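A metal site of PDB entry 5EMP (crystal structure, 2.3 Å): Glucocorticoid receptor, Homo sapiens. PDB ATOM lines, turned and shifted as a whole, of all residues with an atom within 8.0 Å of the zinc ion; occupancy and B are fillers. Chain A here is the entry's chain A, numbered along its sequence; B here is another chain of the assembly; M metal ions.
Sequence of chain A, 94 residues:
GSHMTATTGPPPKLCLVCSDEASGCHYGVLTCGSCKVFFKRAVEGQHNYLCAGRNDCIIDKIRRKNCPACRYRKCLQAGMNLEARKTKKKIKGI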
ATOM      1  N   LEU A  50      14.180 -25.464  -3.536  1.00  0.00           N
ATOM      2  CA  LEU A  50      15.283 -25.438  -2.596  1.00  0.00           C
ATOM      3  C   LEU A  50      16.579 -25.175  -3.325  1.00  0.00           C
ATOM      4  O   LEU A  50      16.940 -25.926  -4.240  1.00  0.00           O
ATOM      5  CB  LEU A  50      15.370 -26.779  -1.853  1.00  0.00           C
ATOM      6  CG  LEU A  50      16.557 -26.878  -0.890  1.00  0.00           C
ATOM      7  CD1 LEU A  50      16.461 -25.768   0.146  1.00  0.00           C
ATOM      8  CD2 LEU A  50      16.603 -28.249  -0.230  1.00  0.00           C
ATOM      9  N   CYS A  51      17.287 -24.116  -2.915  1.00  0.00           N
ATOM     10  CA  CYS A  51      18.612 -23.809  -3.481  1.00  0.00           C
ATOM     11  C   CYS A  51      19.654 -24.852  -3.054  1.00  0.00           C
ATOM     12  O   CYS A  51      19.630 -25.327  -1.934  1.00  0.00           O
ATOM     13  CB  CYS A  51      19.073 -22.430  -2.991  1.00  0.00           C
ATOM     14  SG  CYS A  51      20.670 -21.896  -3.658  1.00  0.00           S
ATOM     15  N   ALA A  52      20.586 -25.216  -3.945  1.00  0.00           N
ATOM     16  CA  ALA A  52      21.609 -26.185  -3.597  1.00  0.00           C
ATOM     17  C   ALA A  52      22.885 -25.467  -3.172  1.00  0.00           C
ATOM     18  O   ALA A  52      23.877 -26.110  -2.835  1.00  0.00           O
ATOM     19  CB  ALA A  52      21.901 -27.131  -4.782  1.00  0.00           C
ATOM     20  N   GLY A  53      22.823 -24.137  -3.191  1.00  0.00           N
ATOM     21  CA  GLY A  53      23.970 -23.297  -2.933  1.00  0.00           C
ATOM     22  C   GLY A  53      23.837 -22.531  -1.640  1.00  0.00           C
ATOM     23  O   GLY A  53      23.774 -23.124  -0.549  1.00  0.00           O
ATOM     24  N   ARG A  54      23.772 -21.204  -1.761  1.00  0.00           N
ATOM     25  CA  ARG A  54      23.689 -20.333  -0.606  1.00  0.00           C
ATOM     26  C   ARG A  54      22.602 -19.272  -0.829  1.00  0.00           C
ATOM     27  O   ARG A  54      22.737 -18.151  -0.344  1.00  0.00           O
ATOM     28  CB  ARG A  54      25.040 -19.667  -0.356  1.00  0.00           C
ATOM     29  CG  ARG A  54      26.200 -20.645  -0.133  1.00  0.00           C
ATOM     30  CD  ARG A  54      27.560 -20.026  -0.490  1.00  0.00           C
ATOM     31  NE  ARG A  54      28.668 -20.829   0.025  1.00  0.00           N
ATOM     32  CZ  ARG A  54      29.211 -21.877  -0.618  1.00  0.00           C
ATOM     33  NH1 ARG A  54      28.755 -22.270  -1.800  1.00  0.00           N
ATOM     34  NH2 ARG A  54      30.218 -22.525  -0.059  1.00  0.00           N
ATOM     35  N   ASN A  55      21.542 -19.624  -1.552  1.00  0.00           N
ATOM     36  CA  ASN A  55      20.468 -18.678  -1.889  1.00  0.00           C
ATOM     37  C   ASN A  55      20.948 -17.408  -2.638  1.00  0.00           C
ATOM     38  O   ASN A  55      20.371 -16.329  -2.489  1.00  0.00           O
ATOM     39  CB  ASN A  55      19.676 -18.262  -0.618  1.00  0.00           C
ATOM     40  CG  ASN A  55      18.481 -19.169  -0.322  1.00  0.00           C
ATOM     41  OD1 ASN A  55      18.065 -19.983  -1.164  1.00  0.00           O
ATOM     42  ND2 ASN A  55      17.916 -19.025   0.872  1.00  0.00           N
ATOM     43  N   ASP A  56      22.010 -17.545  -3.434  1.00  0.00           N
ATOM     44  CA  ASP A  56      22.523 -16.418  -4.225  1.00  0.00           C
ATOM     45  C   ASP A  56      23.098 -16.895  -5.574  1.00  0.00           C
ATOM     46  O   ASP A  56      24.161 -16.430  -5.990  1.00  0.00           O
ATOM     47  CB  ASP A  56      23.602 -15.631  -3.452  1.00  0.00           C
ATOM     48  CG  ASP A  56      24.869 -16.466  -3.197  1.00  0.00           C
ATOM     49  OD1 ASP A  56      24.837 -17.704  -3.397  1.00  0.00           O
ATOM     50  OD2 ASP A  56      25.903 -15.890  -2.803  1.00  0.00           O
ATOM     51  N   CYS A  57      22.413 -17.823  -6.238  1.00  0.00           N
ATOM     52  CA  CYS A  57      22.908 -18.333  -7.512  1.00  0.00           C
ATOM     53  C   CYS A  57      22.964 -17.267  -8.629  1.00  0.00           C
ATOM     54  O   CYS A  57      22.244 -16.248  -8.615  1.00  0.00           O
ATOM     55  CB  CYS A  57      22.101 -19.552  -7.950  1.00  0.00           C
ATOM     56  SG  CYS A  57      22.286 -20.916  -6.816  1.00  0.00           S
ATOM     57  N   ILE A  58      23.847 -17.501  -9.591  1.00  0.00           N
ATOM     58  CA  ILE A  58      23.876 -16.680 -10.804  1.00  0.00           C
ATOM     59  C   ILE A  58      22.766 -17.124 -11.748  1.00  0.00           C
ATOM     60  O   ILE A  58      22.633 -18.326 -12.055  1.00  0.00           O
ATOM     61  CB  ILE A  58      25.243 -16.795 -11.488  1.00  0.00           C
ATOM     62  CG1 ILE A  58      26.321 -16.195 -10.587  1.00  0.00           C
ATOM     63  CG2 ILE A  58      25.231 -16.128 -12.861  1.00  0.00           C
ATOM     64  CD1 ILE A  58      27.707 -16.425 -11.084  1.00  0.00           C
ATOM     65  N   ILE A  59      21.941 -16.183 -12.191  1.00  0.00           N
ATOM     66  CA  ILE A  59      20.831 -16.495 -13.069  1.00  0.00           C
ATOM     67  C   ILE A  59      21.106 -15.993 -14.489  1.00  0.00           C
ATOM     68  O   ILE A  59      21.038 -14.795 -14.749  1.00  0.00           O
ATOM     69  CB  ILE A  59      19.530 -15.881 -12.542  1.00  0.00           C
ATOM     70  CG1 ILE A  59      19.267 -16.351 -11.111  1.00  0.00           C
ATOM     71  CG2 ILE A  59      18.355 -16.266 -13.439  1.00  0.00           C
ATOM     72  CD1 ILE A  59      19.086 -17.889 -10.970  1.00  0.00           C
ATOM     73  N   ARG A  63      22.244 -20.706 -16.813  1.00  0.00           N
ATOM     74  CA  ARG A  63      22.172 -21.086 -15.406  1.00  0.00           C
ATOM     75  C   ARG A  63      20.775 -20.972 -14.757  1.00  0.00           C
ATOM     76  O   ARG A  63      20.551 -21.547 -13.682  1.00  0.00           O
ATOM     77  CB  ARG A  63      23.257 -20.336 -14.609  1.00  0.00           C
ATOM     78  CG  ARG A  63      24.694 -20.601 -15.121  1.00  0.00           C
ATOM     79  CD  ARG A  63      25.789 -19.859 -14.329  1.00  0.00           C
ATOM     80  NE  ARG A  63      26.541 -19.028 -15.265  1.00  0.00           N
ATOM     81  CZ  ARG A  63      27.792 -19.240 -15.647  1.00  0.00           C
ATOM     82  NH1 ARG A  63      28.503 -20.235 -15.144  1.00  0.00           N
ATOM     83  NH2 ARG A  63      28.332 -18.421 -16.527  1.00  0.00           N
ATOM     84  N   ASN A  66      19.148 -24.094 -13.413  1.00  0.00           N
ATOM     85  CA  ASN A  66      19.711 -24.734 -12.257  1.00  0.00           C
ATOM     86  C   ASN A  66      18.965 -24.495 -10.960  1.00  0.00           C
ATOM     87  O   ASN A  66      18.731 -25.397 -10.202  1.00  0.00           O
ATOM     88  CB  ASN A  66      21.120 -24.240 -12.072  1.00  0.00           C
ATOM     89  CG  ASN A  66      22.035 -24.639 -13.202  1.00  0.00           C
ATOM     90  OD1 ASN A  66      21.617 -25.067 -14.237  1.00  0.00           O
ATOM     91  ND2 ASN A  66      23.280 -24.481 -12.975  1.00  0.00           N
ATOM     92  N   CYS A  67      18.629 -23.256 -10.704  1.00  0.00           N
ATOM     93  CA  CYS A  67      18.040 -22.916  -9.418  1.00  0.00           C
ATOM     94  C   CYS A  67      16.753 -22.113  -9.530  1.00  0.00           C
ATOM     95  O   CYS A  67      16.785 -20.883  -9.541  1.00  0.00           O
ATOM     96  CB  CYS A  67      19.053 -22.185  -8.550  1.00  0.00           C
ATOM     97  SG  CYS A  67      18.560 -22.124  -6.829  1.00  0.00           S
ATOM     98  N   PRO A  68      15.611 -22.809  -9.594  1.00  0.00           N
ATOM     99  CA  PRO A  68      14.277 -22.186  -9.598  1.00  0.00           C
ATOM    100  C   PRO A  68      14.092 -21.342  -8.346  1.00  0.00           C
ATOM    101  O   PRO A  68      13.427 -20.305  -8.415  1.00  0.00           O
ATOM    102  CB  PRO A  68      13.314 -23.384  -9.552  1.00  0.00           C
ATOM    103  CG  PRO A  68      14.112 -24.584  -9.940  1.00  0.00           C
ATOM    104  CD  PRO A  68      15.547 -24.293  -9.609  1.00  0.00           C
ATOM    105  N   ALA A  69      14.669 -21.767  -7.231  1.00  0.00           N
ATOM    106  CA  ALA A  69      14.534 -21.003  -5.989  1.00  0.00           C
ATOM    107  C   ALA A  69      15.187 -19.626  -6.117  1.00  0.00           C
ATOM    108  O   ALA A  69      14.614 -18.624  -5.688  1.00  0.00           O
ATOM    109  CB  ALA A  69      15.115 -21.751  -4.796  1.00  0.00           C
ATOM    110  N   CYS A  70      16.361 -19.578  -6.723  1.00  0.00           N
ATOM    111  CA  CYS A  70      17.042 -18.300  -6.891  1.00  0.00           C
ATOM    112  C   CYS A  70      16.434 -17.481  -8.022  1.00  0.00           C
ATOM    113  O   CYS A  70      16.378 -16.257  -7.974  1.00  0.00           O
ATOM    114  CB  CYS A  70      18.546 -18.495  -7.074  1.00  0.00           C
ATOM    115  SG  CYS A  70      19.417 -18.794  -5.507  1.00  0.00           S
ATOM    116  N   ARG A  71      15.951 -18.180  -9.047  1.00  0.00           N
ATOM    117  CA  ARG A  71      15.301 -17.505 -10.163  1.00  0.00           C
ATOM    118  C   ARG A  71      13.997 -16.830  -9.705  1.00  0.00           C
ATOM    119  O   ARG A  71      13.731 -15.686 -10.054  1.00  0.00           O
ATOM    120  CB  ARG A  71      15.038 -18.476 -11.295  1.00  0.00           C
ATOM    121  CG  ARG A  71      14.519 -17.871 -12.584  1.00  0.00           C
ATOM    122  CD  ARG A  71      14.175 -18.990 -13.593  1.00  0.00           C
ATOM    123  NE  ARG A  71      13.863 -18.463 -14.926  1.00  0.00           N
ATOM    124  CZ  ARG A  71      13.514 -19.203 -15.971  1.00  0.00           C
ATOM    125  NH1 ARG A  71      13.417 -20.517 -15.842  1.00  0.00           N
ATOM    126  NH2 ARG A  71      13.262 -18.626 -17.131  1.00  0.00           N
ATOM    127  N   ARG A  73      13.201 -15.980  -6.626  1.00  0.00           N
ATOM    128  CA  ARG A  73      13.605 -14.904  -5.726  1.00  0.00           C
ATOM    129  C   ARG A  73      14.020 -13.669  -6.527  1.00  0.00           C
ATOM    130  O   ARG A  73      13.588 -12.548  -6.230  1.00  0.00           O
ATOM    131  CB  ARG A  73      14.724 -15.363  -4.780  1.00  0.00           C
ATOM    132  CG  ARG A  73      15.448 -14.252  -4.017  1.00  0.00           C
ATOM    133  CD  ARG A  73      16.336 -14.813  -2.877  1.00  0.00           C
ATOM    134  NE  ARG A  73      17.001 -16.066  -3.255  1.00  0.00           N
ATOM    135  CZ  ARG A  73      16.593 -17.280  -2.882  1.00  0.00           C
ATOM    136  NH1 ARG A  73      15.519 -17.418  -2.102  1.00  0.00           N
ATOM    137  NH2 ARG A  73      17.247 -18.362  -3.287  1.00  0.00           N
ATOM    138  N   ALA B  52      25.868 -22.562 -11.102  1.00  0.00           N
ATOM    139  CA  ALA B  52      25.333 -21.220 -10.818  1.00  0.00           C
ATOM    140  C   ALA B  52      25.797 -20.733  -9.458  1.00  0.00           C
ATOM    141  O   ALA B  52      25.559 -19.585  -9.079  1.00  0.00           O
ATOM    142  CB  ALA B  52      23.816 -21.246 -10.843  1.00  0.00           C
ATOM    143  N   GLY B  53      26.430 -21.634  -8.703  1.00  0.00           N
ATOM    144  CA  GLY B  53      26.907 -21.310  -7.377  1.00  0.00           C
ATOM    145  C   GLY B  53      28.416 -21.225  -7.376  1.00  0.00           C
ATOM    146  O   GLY B  53      28.976 -20.563  -8.235  1.00  0.00           O
ATOM    147  N   CYS B  57      27.981 -27.235  -4.933  1.00  0.00           N
ATOM    148  CA  CYS B  57      26.564 -27.361  -4.649  1.00  0.00           C
ATOM    149  C   CYS B  57      26.278 -28.635  -3.846  1.00  0.00           C
ATOM    150  O   CYS B  57      26.973 -29.638  -4.026  1.00  0.00           O
ATOM    151  CB  CYS B  57      25.749 -27.344  -5.946  1.00  0.00           C
ATOM    152  SG  CYS B  57      25.836 -25.754  -6.870  1.00  0.00           S
ATOM    153  N   ASN B  66      19.600 -30.004  -9.446  1.00  0.00           N
ATOM    154  CA  ASN B  66      19.894 -28.566  -9.567  1.00  0.00           C
ATOM    155  C   ASN B  66      21.183 -28.270 -10.334  1.00  0.00           C
ATOM    156  O   ASN B  66      21.239 -27.375 -11.173  1.00  0.00           O
ATOM    157  CB  ASN B  66      19.996 -27.868  -8.197  1.00  0.00           C
ATOM    158  CG  ASN B  66      18.685 -27.883  -7.413  1.00  0.00           C
ATOM    159  OD1 ASN B  66      17.858 -28.780  -7.582  1.00  0.00           O
ATOM    160  ND2 ASN B  66      18.513 -26.888  -6.545  1.00  0.00           N
HETATM  161 ZN    ZN M   1      20.244 -20.962  -5.735  1.00  0.00          ZN
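The side-chain sulfur (SG) of Cys 51 sits close to the backbone NH (N) of Asn 55, at 3.2 Å. SG of Cys 51 sits close to N of Gly 53 of chain A. SG of Cys 51 sits close to N of Arg 54 (3.7 Å). The side-chain sulfur (SG) of Cys 70 lies close to the backbone NH (N) of Asp 56, 3.5 Å away. NH2 of Arg 73 lies close to SG of Cys 70 (3.1 Å).
Within 4 Å of the zinc ion: Cys 51, Cys 57 of chain A, Cys 67 and Cys 70. The nearest printed residue that does not touch the zinc ion is Asn 55 (4.5 Å).
The zinc ion is bound by the side-chain sulfur (SG) of Cys 57 of chain A, at 2.3 Å. The zinc ion is bound by SG of Cys 51, 2.3 Å away. SG of Cys 67 is bound to the zinc ion (2.3 Å). The zinc ion is bound by SG of Cys 70 (2.3 Å).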
